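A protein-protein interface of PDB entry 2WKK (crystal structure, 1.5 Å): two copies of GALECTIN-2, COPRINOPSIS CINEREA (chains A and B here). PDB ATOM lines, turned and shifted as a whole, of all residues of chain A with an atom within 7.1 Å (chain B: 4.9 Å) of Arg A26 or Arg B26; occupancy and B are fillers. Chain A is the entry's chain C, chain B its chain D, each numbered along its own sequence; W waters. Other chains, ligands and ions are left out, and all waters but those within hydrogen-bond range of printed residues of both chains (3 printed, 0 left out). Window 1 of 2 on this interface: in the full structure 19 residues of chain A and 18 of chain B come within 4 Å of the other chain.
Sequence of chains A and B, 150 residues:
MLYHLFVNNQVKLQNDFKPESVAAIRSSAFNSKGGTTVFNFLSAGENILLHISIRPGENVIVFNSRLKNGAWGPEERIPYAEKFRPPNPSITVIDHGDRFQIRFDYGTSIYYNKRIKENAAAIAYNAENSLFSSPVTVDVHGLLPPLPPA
Arg B26 touches three residues of chain A. Of the printed residues of chain B, Pro A135 touches His B4. Of the printed residues of chain B, Ser A27 touches Leu B2. Of the printed residues of chain A, Ser B27 touches Leu A2. Ala A29 touches none of the printed residues of chain B. Val A136 touches none of the printed residues of chain B. The nearest printed residue of chain B that does not touch Pro A135 is Thr B137 (6.7 Å).
Leu A2 touches Arg B26, and with the chains exchanged Arg A26 touches Leu B2. Leu A2 touches Ser B27, and with the chains exchanged Ser A27 touches Leu B2. Leu A2 touches Ser B28, and with the chains exchanged Ser A28 touches Leu B2. His A4 touches Ser B28, and with the chains exchanged Ser A28 touches His B4. 13 positions are printed for both chains.
Hydrophobic or aromatic side chains of chain A within 4 Å of the printed part of chain B: Leu A2 and His A4. Among the printed residues, 18 pairs touch across the chains.
OG of Ser B28 is in hydrogen-bond range of ND1 of His A4 (2.8 Å). NE2 of His A4 lies within hydrogen-bond range of OG1 of Thr B137, at 2.7 Å. The side-chain carboxylate (OD2) of Asp B139 lies within salt-bridge range of the guanidinium group (NH1) of Arg A26, at 2.8 Å. OG of Ser A28 lies within hydrogen-bond range of ND1 of His B4. The backbone NH of Leu B2 lies within hydrogen-bond range of the side-chain amide oxygen of Asn A88, 2.8 Å away. The backbone carbonyl oxygen of Pro A135 lies close to a ring nitrogen (ND1) of His B4, at 3.3 Å. A ring nitrogen (NE2) of His B4 lies within hydrogen-bond range of the side-chain hydroxyl (OG1) of Thr A137. The side-chain hydroxyl of Thr A137 is in hydrogen-bond range of the side-chain hydroxyl of Thr B137, at 2.7 Å. The side-chain carboxylate (OD2) of Asp A139 is in salt-bridge range of the guanidinium group (NH1) of Arg B26 (2.8 Å).
Among the printed residues, merely in contact across the chains: Leu A2 with Arg B26 (3.7 Å), Leu A2 with Ser B27 (3.7 Å), Leu A2 with Ser B28 (3.6 Å), His A4 with Ser B133 (3.5 Å), Arg A26 with Leu B2 (3.7 Å), Arg A26 with Arg B26 (3.5 Å), Ser A27 with Leu B2 (3.6 Å), Ser A28 with Leu B2 (3.7 Å) and Ser A133 with His B4 (3.5 Å).
Water W2 bridges the backbone carbonyl oxygen of Leu B2 and the backbone carbonyl oxygen of Ser A28. Water W3 bridges the backbone carbonyl oxygen (O) of Leu A2 and the backbone carbonyl oxygen (O) of Ser B28. Water W1 lies within hydrogen-bond range of the side-chain carboxylate (OD1) of Asp A139, the guanidinium group (NH2) of Arg A26 and the guanidinium group (NH2) of Arg B26.
The side-chain hydroxyl of Ser A27 lies within hydrogen-bond range of the backbone carbonyl oxygen of Ala A29, at 2.6 Å. The backbone carbonyl oxygen of Pro A89 is in hydrogen-bond range of the backbone NH of Ser A27 (3.0 Å). The backbone NH (N) of Ser A28 is in hydrogen-bond range of the side-chain hydroxyl (OG) of Ser A133, 3.0 Å away. OG of Ser A133 lies within hydrogen-bond range of O of Pro A135, at 2.8 Å. The backbone carbonyl oxygen (O) of Thr B137 lies within hydrogen-bond range of the backbone NH (N) of Arg B26. The side-chain hydroxyl (OG) of Ser B27 lies within hydrogen-bond range of the backbone NH (N) of Ser B133, 2.9 Å away.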
ATOM      1  N   MET A   1      24.642  20.837 -36.496  1.00  0.00           N
ATOM      2  CA  MET A   1      25.728  20.376 -35.639  1.00  0.00           C
ATOM      3  C   MET A   1      26.008  21.405 -34.557  1.00  0.00           C
ATOM      4  O   MET A   1      26.170  22.589 -34.856  1.00  0.00           O
ATOM      5  CB  MET A   1      26.995  20.132 -36.462  1.00  0.00           C
ATOM      6  CG  MET A   1      28.176  19.604 -35.653  1.00  0.00           C
ATOM      7  SD  MET A   1      27.913  17.918 -35.070  1.00  0.00           S
ATOM      8  CE  MET A   1      27.600  17.100 -36.632  1.00  0.00           C
ATOM      9  N   LEU A   2      26.080  20.945 -33.310  1.00  0.00           N
ATOM     10  CA  LEU A   2      26.306  21.817 -32.164  1.00  0.00           C
ATOM     11  C   LEU A   2      27.782  21.819 -31.791  1.00  0.00           C
ATOM     12  O   LEU A   2      28.383  20.752 -31.644  1.00  0.00           O
ATOM     13  CB  LEU A   2      25.478  21.351 -30.956  1.00  0.00           C
ATOM     14  CG  LEU A   2      25.764  22.055 -29.626  1.00  0.00           C
ATOM     15  CD1 LEU A   2      25.420  23.548 -29.696  1.00  0.00           C
ATOM     16  CD2 LEU A   2      25.004  21.391 -28.480  1.00  0.00           C
ATOM     17  N   TYR A   3      28.360  23.013 -31.662  1.00  0.00           N
ATOM     18  CA  TYR A   3      29.715  23.182 -31.152  1.00  0.00           C
ATOM     19  C   TYR A   3      29.719  24.096 -29.944  1.00  0.00           C
ATOM     20  O   TYR A   3      28.895  25.015 -29.830  1.00  0.00           O
ATOM     21  CB  TYR A   3      30.626  23.824 -32.198  1.00  0.00           C
ATOM     22  CG  TYR A   3      30.693  23.081 -33.506  1.00  0.00           C
ATOM     23  CD1 TYR A   3      29.745  23.307 -34.499  1.00  0.00           C
ATOM     24  CD2 TYR A   3      31.709  22.167 -33.760  1.00  0.00           C
ATOM     25  CE1 TYR A   3      29.802  22.643 -35.710  1.00  0.00           C
ATOM     26  CE2 TYR A   3      31.771  21.490 -34.963  1.00  0.00           C
ATOM     27  CZ  TYR A   3      30.820  21.739 -35.939  1.00  0.00           C
ATOM     28  OH  TYR A   3      30.881  21.063 -37.134  1.00  0.00           O
ATOM     29  N   HIS A   4      30.667  23.855 -29.047  1.00  0.00           N
ATOM     30  CA  HIS A   4      30.951  24.801 -27.986  1.00  0.00           C
ATOM     31  C   HIS A   4      32.290  25.462 -28.266  1.00  0.00           C
ATOM     32  O   HIS A   4      33.351  24.838 -28.175  1.00  0.00           O
ATOM     33  CB  HIS A   4      30.913  24.122 -26.618  1.00  0.00           C
ATOM     34  CG  HIS A   4      29.526  23.772 -26.177  1.00  0.00           C
ATOM     35  ND1 HIS A   4      29.168  22.508 -25.765  1.00  0.00           N
ATOM     36  CD2 HIS A   4      28.403  24.523 -26.099  1.00  0.00           C
ATOM     37  CE1 HIS A   4      27.886  22.494 -25.447  1.00  0.00           C
ATOM     38  NE2 HIS A   4      27.397  23.704 -25.645  1.00  0.00           N
ATOM     39  N   ALA A  24      24.614  29.768 -36.381  1.00  0.00           N
ATOM     40  CA  ALA A  24      23.911  30.538 -35.364  1.00  0.00           C
ATOM     41  C   ALA A  24      24.709  30.515 -34.072  1.00  0.00           C
ATOM     42  O   ALA A  24      24.735  29.502 -33.378  1.00  0.00           O
ATOM     43  CB  ALA A  24      22.514  29.976 -35.130  1.00  0.00           C
ATOM     44  N   ILE A  25      25.349  31.641 -33.764  1.00  0.00           N
ATOM     45  CA  ILE A  25      26.160  31.801 -32.566  1.00  0.00           C
ATOM     46  C   ILE A  25      25.326  32.469 -31.485  1.00  0.00           C
ATOM     47  O   ILE A  25      24.727  33.518 -31.725  1.00  0.00           O
ATOM     48  CB  ILE A  25      27.400  32.684 -32.860  1.00  0.00           C
ATOM     49  CG1 ILE A  25      28.243  32.053 -33.976  1.00  0.00           C
ATOM     50  CG2 ILE A  25      28.229  32.911 -31.589  1.00  0.00           C
ATOM     51  CD1 ILE A  25      29.256  33.014 -34.599  1.00  0.00           C
ATOM     52  N   ARG A  26      25.271  31.855 -30.304  1.00  0.00           N
ATOM     53  CA  ARG A  26      24.484  32.400 -29.210  1.00  0.00           C
ATOM     54  C   ARG A  26      25.271  32.409 -27.914  1.00  0.00           C
ATOM     55  O   ARG A  26      25.915  31.419 -27.561  1.00  0.00           O
ATOM     56  CB  ARG A  26      23.191  31.600 -29.023  1.00  0.00           C
ATOM     57  CG  ARG A  26      22.287  31.621 -30.250  1.00  0.00           C
ATOM     58  CD  ARG A  26      20.944  30.963 -29.973  1.00  0.00           C
ATOM     59  NE  ARG A  26      21.031  29.523 -29.727  1.00  0.00           N
ATOM     60  CZ  ARG A  26      20.566  28.910 -28.637  1.00  0.00           C
ATOM     61  NH1 ARG A  26      19.987  29.615 -27.667  1.00  0.00           N
ATOM     62  NH2 ARG A  26      20.669  27.585 -28.521  1.00  0.00           N
ATOM     63  N   SER A  27      25.200  33.529 -27.207  1.00  0.00           N
ATOM     64  CA  SER A  27      25.893  33.701 -25.934  1.00  0.00           C
ATOM     65  C   SER A  27      24.923  33.556 -24.762  1.00  0.00           C
ATOM     66  O   SER A  27      23.770  33.996 -24.838  1.00  0.00           O
ATOM     67  CB  SER A  27      26.544  35.088 -25.898  1.00  0.00           C
ATOM     68  OG  SER A  27      27.175  35.325 -24.661  1.00  0.00           O
ATOM     69  N   SER A  28      25.390  32.945 -23.674  1.00  0.00           N
ATOM     70  CA  SER A  28      24.569  32.822 -22.469  1.00  0.00           C
ATOM     71  C   SER A  28      24.662  34.071 -21.592  1.00  0.00           C
ATOM     72  O   SER A  28      23.969  34.178 -20.577  1.00  0.00           O
ATOM     73  CB  SER A  28      24.967  31.587 -21.656  1.00  0.00           C
ATOM     74  OG  SER A  28      26.335  31.638 -21.285  1.00  0.00           O
ATOM     75  N   ALA A  29      25.514  35.015 -21.980  1.00  0.00           N
ATOM     76  CA  ALA A  29      25.682  36.232 -21.198  1.00  0.00           C
ATOM     77  C   ALA A  29      26.022  37.441 -22.061  1.00  0.00           C
ATOM     78  O   ALA A  29      26.422  37.316 -23.223  1.00  0.00           O
ATOM     79  CB  ALA A  29      26.764  36.028 -20.152  1.00  0.00           C
ATOM     80  N   ASN A  88      21.167  37.217 -23.787  1.00  0.00           N
ATOM     81  CA  ASN A  88      21.559  36.168 -24.726  1.00  0.00           C
ATOM     82  C   ASN A  88      21.781  36.741 -26.126  1.00  0.00           C
ATOM     83  O   ASN A  88      21.001  36.463 -27.040  1.00  0.00           O
ATOM     84  CB  ASN A  88      20.469  35.097 -24.849  1.00  0.00           C
ATOM     85  CG  ASN A  88      20.241  34.291 -23.570  1.00  0.00           C
ATOM     86  OD1 ASN A  88      19.229  33.611 -23.465  1.00  0.00           O
ATOM     87  ND2 ASN A  88      21.168  34.351 -22.617  1.00  0.00           N
ATOM     88  N   PRO A  89      22.843  37.537 -26.304  1.00  0.00           N
ATOM     89  CA  PRO A  89      23.062  38.148 -27.620  1.00  0.00           C
ATOM     90  C   PRO A  89      23.450  37.095 -28.645  1.00  0.00           C
ATOM     91  O   PRO A  89      23.903  36.004 -28.259  1.00  0.00           O
ATOM     92  CB  PRO A  89      24.225  39.117 -27.379  1.00  0.00           C
ATOM     93  CG  PRO A  89      24.909  38.601 -26.149  1.00  0.00           C
ATOM     94  CD  PRO A  89      23.873  37.909 -25.319  1.00  0.00           C
ATOM     95  N   SER A  90      23.263  37.403 -29.927  1.00  0.00           N
ATOM     96  CA  SER A  90      23.528  36.431 -30.989  1.00  0.00           C
ATOM     97  C   SER A  90      24.202  37.054 -32.201  1.00  0.00           C
ATOM     98  O   SER A  90      24.139  38.265 -32.400  1.00  0.00           O
ATOM     99  CB  SER A  90      22.238  35.737 -31.437  1.00  0.00           C
ATOM    100  OG  SER A  90      21.441  36.599 -32.235  1.00  0.00           O
ATOM    101  N   ILE A  91      24.840  36.196 -32.995  1.00  0.00           N
ATOM    102  CA  ILE A  91      25.384  36.543 -34.304  1.00  0.00           C
ATOM    103  C   ILE A  91      25.031  35.385 -35.229  1.00  0.00           C
ATOM    104  O   ILE A  91      25.307  34.219 -34.913  1.00  0.00           O
ATOM    105  CB  ILE A  91      26.914  36.660 -34.275  1.00  0.00           C
ATOM    106  CG1 ILE A  91      27.377  37.663 -33.216  1.00  0.00           C
ATOM    107  CG2 ILE A  91      27.455  37.047 -35.656  1.00  0.00           C
ATOM    108  CD1 ILE A  91      28.887  37.638 -32.997  1.00  0.00           C
ATOM    109  N   THR A  92      24.405  35.691 -36.359  1.00  0.00           N
ATOM    110  CA  THR A  92      24.061  34.657 -37.321  1.00  0.00           C
ATOM    111  C   THR A  92      24.768  34.954 -38.636  1.00  0.00           C
ATOM    112  O   THR A  92      24.657  36.060 -39.177  1.00  0.00           O
ATOM    113  CB  THR A  92      22.534  34.558 -37.512  1.00  0.00           C
ATOM    114  OG1 THR A  92      21.924  34.279 -36.241  1.00  0.00           O
ATOM    115  CG2 THR A  92      22.178  33.437 -38.486  1.00  0.00           C
ATOM    116  N   PHE A 132      30.986  38.358 -24.505  1.00  0.00           N
ATOM    117  CA  PHE A 132      30.095  37.199 -24.499  1.00  0.00           C
ATOM    118  C   PHE A 132      30.596  36.080 -23.598  1.00  0.00           C
ATOM    119  O   PHE A 132      31.694  36.160 -23.039  1.00  0.00           O
ATOM    120  CB  PHE A 132      29.901  36.673 -25.926  1.00  0.00           C
ATOM    121  CG  PHE A 132      29.505  37.735 -26.910  1.00  0.00           C
ATOM    122  CD1 PHE A 132      30.232  37.932 -28.078  1.00  0.00           C
ATOM    123  CD2 PHE A 132      28.421  38.558 -26.655  1.00  0.00           C
ATOM    124  CE1 PHE A 132      29.871  38.932 -28.979  1.00  0.00           C
ATOM    125  CE2 PHE A 132      28.050  39.556 -27.554  1.00  0.00           C
ATOM    126  CZ  PHE A 132      28.778  39.741 -28.717  1.00  0.00           C
ATOM    127  N   SER A 133      29.786  35.035 -23.478  1.00  0.00           N
ATOM    128  CA  SER A 133      30.124  33.899 -22.629  1.00  0.00           C
ATOM    129  C   SER A 133      31.252  33.076 -23.225  1.00  0.00           C
ATOM    130  O   SER A 133      31.548  33.177 -24.421  1.00  0.00           O
ATOM    131  CB  SER A 133      28.898  33.006 -22.417  1.00  0.00           C
ATOM    132  OG  SER A 133      28.385  32.519 -23.653  1.00  0.00           O
ATOM    133  N   PRO A 135      31.949  28.975 -23.143  1.00  0.00           N
ATOM    134  CA  PRO A 135      31.923  29.087 -24.601  1.00  0.00           C
ATOM    135  C   PRO A 135      30.708  29.863 -25.087  1.00  0.00           C
ATOM    136  O   PRO A 135      29.850  30.251 -24.285  1.00  0.00           O
ATOM    137  CB  PRO A 135      31.775  27.626 -25.023  1.00  0.00           C
ATOM    138  CG  PRO A 135      30.842  27.054 -23.968  1.00  0.00           C
ATOM    139  CD  PRO A 135      31.303  27.730 -22.676  1.00  0.00           C
ATOM    140  N   VAL A 136      30.653  30.102 -26.394  1.00  0.00           N
ATOM    141  CA  VAL A 136      29.380  30.377 -27.034  1.00  0.00           C
ATOM    142  C   VAL A 136      28.824  29.096 -27.662  1.00  0.00           C
ATOM    143  O   VAL A 136      29.569  28.180 -28.037  1.00  0.00           O
ATOM    144  CB  VAL A 136      29.486  31.495 -28.098  1.00  0.00           C
ATOM    145  CG1 VAL A 136      29.753  32.830 -27.426  1.00  0.00           C
ATOM    146  CG2 VAL A 136      30.582  31.174 -29.125  1.00  0.00           C
ATOM    147  N   THR A 137      27.504  29.029 -27.747  1.00  0.00           N
ATOM    148  CA  THR A 137      26.826  27.935 -28.423  1.00  0.00           C
ATOM    149  C   THR A 137      26.806  28.229 -29.916  1.00  0.00           C
ATOM    150  O   THR A 137      26.428  29.320 -30.332  1.00  0.00           O
ATOM    151  CB  THR A 137      25.375  27.806 -27.891  1.00  0.00           C
ATOM    152  OG1 THR A 137      25.403  27.187 -26.598  1.00  0.00           O
ATOM    153  CG2 THR A 137      24.507  26.988 -28.824  1.00  0.00           C
ATOM    154  N   VAL A 138      27.224  27.268 -30.731  1.00  0.00           N
ATOM    155  CA  VAL A 138      27.190  27.464 -32.178  1.00  0.00           C
ATOM    156  C   VAL A 138      26.468  26.301 -32.834  1.00  0.00           C
ATOM    157  O   VAL A 138      26.907  25.158 -32.721  1.00  0.00           O
ATOM    158  CB  VAL A 138      28.603  27.567 -32.777  1.00  0.00           C
ATOM    159  CG1 VAL A 138      28.525  27.999 -34.249  1.00  0.00           C
ATOM    160  CG2 VAL A 138      29.450  28.548 -31.976  1.00  0.00           C
ATOM    161  N   ASP A 139      25.359  26.585 -33.513  1.00  0.00           N
ATOM    162  CA  ASP A 139      24.696  25.562 -34.316  1.00  0.00           C
ATOM    163  C   ASP A 139      24.987  25.845 -35.775  1.00  0.00           C
ATOM    164  O   ASP A 139      24.716  26.945 -36.259  1.00  0.00           O
ATOM    165  CB  ASP A 139      23.183  25.530 -34.070  1.00  0.00           C
ATOM    166  CG  ASP A 139      22.828  24.889 -32.750  1.00  0.00           C
ATOM    167  OD1 ASP A 139      22.469  25.627 -31.807  1.00  0.00           O
ATOM    168  OD2 ASP A 139      22.930  23.649 -32.648  1.00  0.00           O
ATOM    169  N   LEU B   2      18.928  30.944 -22.612  1.00  0.00           N
ATOM    170  CA  LEU B   2      20.079  30.064 -22.825  1.00  0.00           C
ATOM    171  C   LEU B   2      20.990  30.068 -21.600  1.00  0.00           C
ATOM    172  O   LEU B   2      21.363  31.133 -21.099  1.00  0.00           O
ATOM    173  CB  LEU B   2      20.881  30.527 -24.056  1.00  0.00           C
ATOM    174  CG  LEU B   2      22.237  29.835 -24.272  1.00  0.00           C
ATOM    175  CD1 LEU B   2      22.062  28.341 -24.531  1.00  0.00           C
ATOM    176  CD2 LEU B   2      23.024  30.471 -25.417  1.00  0.00           C
ATOM    177  N   HIS B   4      24.619  27.994 -20.005  1.00  0.00           N
ATOM    178  CA  HIS B   4      25.690  27.025 -20.166  1.00  0.00           C
ATOM    179  C   HIS B   4      25.928  26.381 -18.812  1.00  0.00           C
ATOM    180  O   HIS B   4      26.421  27.017 -17.872  1.00  0.00           O
ATOM    181  CB  HIS B   4      26.961  27.672 -20.711  1.00  0.00           C
ATOM    182  CG  HIS B   4      26.860  28.044 -22.158  1.00  0.00           C
ATOM    183  ND1 HIS B   4      27.190  29.294 -22.629  1.00  0.00           N
ATOM    184  CD2 HIS B   4      26.457  27.331 -23.236  1.00  0.00           C
ATOM    185  CE1 HIS B   4      26.993  29.339 -23.934  1.00  0.00           C
ATOM    186  NE2 HIS B   4      26.550  28.162 -24.329  1.00  0.00           N
ATOM    187  N   ALA B  24      15.511  22.144 -22.832  1.00  0.00           N
ATOM    188  CA  ALA B  24      16.166  21.381 -23.888  1.00  0.00           C
ATOM    189  C   ALA B  24      17.667  21.376 -23.634  1.00  0.00           C
ATOM    190  O   ALA B  24      18.353  22.379 -23.860  1.00  0.00           O
ATOM    191  CB  ALA B  24      15.856  21.981 -25.252  1.00  0.00           C
ATOM    192  N   ILE B  25      18.166  20.248 -23.140  1.00  0.00           N
ATOM    193  CA  ILE B  25      19.587  20.098 -22.845  1.00  0.00           C
ATOM    194  C   ILE B  25      20.266  19.438 -24.036  1.00  0.00           C
ATOM    195  O   ILE B  25      19.826  18.391 -24.501  1.00  0.00           O
ATOM    196  CB  ILE B  25      19.783  19.216 -21.592  1.00  0.00           C
ATOM    197  CG1 ILE B  25      19.100  19.857 -20.380  1.00  0.00           C
ATOM    198  CG2 ILE B  25      21.265  18.972 -21.325  1.00  0.00           C
ATOM    199  CD1 ILE B  25      18.875  18.889 -19.210  1.00  0.00           C
ATOM    200  N   ARG B  26      21.336  20.052 -24.534  1.00  0.00           N
ATOM    201  CA  ARG B  26      22.055  19.503 -25.671  1.00  0.00           C
ATOM    202  C   ARG B  26      23.559  19.476 -25.428  1.00  0.00           C
ATOM    203  O   ARG B  26      24.150  20.462 -24.978  1.00  0.00           O
ATOM    204  CB  ARG B  26      21.747  20.311 -26.932  1.00  0.00           C
ATOM    205  CG  ARG B  26      20.275  20.309 -27.292  1.00  0.00           C
ATOM    206  CD  ARG B  26      20.022  20.936 -28.656  1.00  0.00           C
ATOM    207  NE  ARG B  26      20.302  22.373 -28.689  1.00  0.00           N
ATOM    208  CZ  ARG B  26      21.114  22.969 -29.567  1.00  0.00           C
ATOM    209  NH1 ARG B  26      21.761  22.253 -30.484  1.00  0.00           N
ATOM    210  NH2 ARG B  26      21.281  24.285 -29.521  1.00  0.00           N
ATOM    211  N   SER B  27      24.173  18.343 -25.744  1.00  0.00           N
ATOM    212  CA  SER B  27      25.610  18.177 -25.581  1.00  0.00           C
ATOM    213  C   SER B  27      26.322  18.313 -26.926  1.00  0.00           C
ATOM    214  O   SER B  27      25.805  17.870 -27.943  1.00  0.00           O
ATOM    215  CB  SER B  27      25.900  16.798 -24.980  1.00  0.00           C
ATOM    216  OG  SER B  27      27.290  16.547 -24.908  1.00  0.00           O
ATOM    217  N   SER B  28      27.510  18.913 -26.929  1.00  0.00           N
ATOM    218  CA  SER B  28      28.302  18.995 -28.155  1.00  0.00           C
ATOM    219  C   SER B  28      29.132  17.734 -28.408  1.00  0.00           C
ATOM    220  O   SER B  28      29.810  17.630 -29.430  1.00  0.00           O
ATOM    221  CB  SER B  28      29.212  20.225 -28.141  1.00  0.00           C
ATOM    222  OG  SER B  28      30.111  20.182 -27.048  1.00  0.00           O
ATOM    223  N   PRO B  89      24.172  14.322 -28.306  1.00  0.00           N
ATOM    224  CA  PRO B  89      23.020  13.740 -27.609  1.00  0.00           C
ATOM    225  C   PRO B  89      22.240  14.792 -26.831  1.00  0.00           C
ATOM    226  O   PRO B  89      22.772  15.864 -26.520  1.00  0.00           O
ATOM    227  CB  PRO B  89      23.666  12.732 -26.649  1.00  0.00           C
ATOM    228  CG  PRO B  89      25.060  13.227 -26.462  1.00  0.00           C
ATOM    229  CD  PRO B  89      25.446  13.763 -27.822  1.00  0.00           C
ATOM    230  N   SER B  90      20.989  14.483 -26.510  1.00  0.00           N
ATOM    231  CA  SER B  90      20.117  15.467 -25.887  1.00  0.00           C
ATOM    232  C   SER B  90      19.186  14.861 -24.859  1.00  0.00           C
ATOM    233  O   SER B  90      18.917  13.651 -24.870  1.00  0.00           O
ATOM    234  CB  SER B  90      19.276  16.188 -26.949  1.00  0.00           C
ATOM    235  OG  SER B  90      18.233  15.349 -27.424  1.00  0.00           O
ATOM    236  N   SER B 133      29.392  16.845 -22.931  1.00  0.00           N
ATOM    237  CA  SER B 133      30.284  17.996 -22.910  1.00  0.00           C
ATOM    238  C   SER B 133      30.149  18.809 -21.623  1.00  0.00           C
ATOM    239  O   SER B 133      29.161  18.698 -20.902  1.00  0.00           O
ATOM    240  CB  SER B 133      30.001  18.887 -24.122  1.00  0.00           C
ATOM    241  OG  SER B 133      28.655  19.341 -24.121  1.00  0.00           O
ATOM    242  N   VAL B 136      26.970  21.791 -21.047  1.00  0.00           N
ATOM    243  CA  VAL B 136      25.904  21.475 -21.991  1.00  0.00           C
ATOM    244  C   VAL B 136      25.144  22.767 -22.273  1.00  0.00           C
ATOM    245  O   VAL B 136      25.104  23.687 -21.437  1.00  0.00           O
ATOM    246  CB  VAL B 136      24.944  20.354 -21.494  1.00  0.00           C
ATOM    247  CG1 VAL B 136      25.647  19.003 -21.538  1.00  0.00           C
ATOM    248  CG2 VAL B 136      24.427  20.651 -20.087  1.00  0.00           C
ATOM    249  N   THR B 137      24.578  22.847 -23.469  1.00  0.00           N
ATOM    250  CA  THR B 137      23.705  23.948 -23.843  1.00  0.00           C
ATOM    251  C   THR B 137      22.319  23.656 -23.283  1.00  0.00           C
ATOM    252  O   THR B 137      21.787  22.561 -23.467  1.00  0.00           O
ATOM    253  CB  THR B 137      23.639  24.096 -25.380  1.00  0.00           C
ATOM    254  OG1 THR B 137      24.849  24.707 -25.840  1.00  0.00           O
ATOM    255  CG2 THR B 137      22.436  24.946 -25.818  1.00  0.00           C
ATOM    256  N   ASP B 139      18.488  25.338 -23.243  1.00  0.00           N
ATOM    257  CA  ASP B 139      17.479  26.347 -23.548  1.00  0.00           C
ATOM    258  C   ASP B 139      16.227  26.072 -22.723  1.00  0.00           C
ATOM    259  O   ASP B 139      15.641  24.991 -22.818  1.00  0.00           O
ATOM    260  CB  ASP B 139      17.147  26.366 -25.043  1.00  0.00           C
ATOM    261  CG  ASP B 139      18.241  27.010 -25.867  1.00  0.00           C
ATOM    262  OD1 ASP B 139      18.952  26.273 -26.584  1.00  0.00           O
ATOM    263  OD2 ASP B 139      18.395  28.252 -25.786  1.00  0.00           O
HETATM  264  O   HOH W   1      19.685  26.560 -31.324  1.00  0.00           O
HETATM  265  O   HOH W   2      22.648  32.320 -18.988  1.00  0.00           O
HETATM  266  O   HOH W   3      30.805  19.484 -31.256  1.00  0.00           O
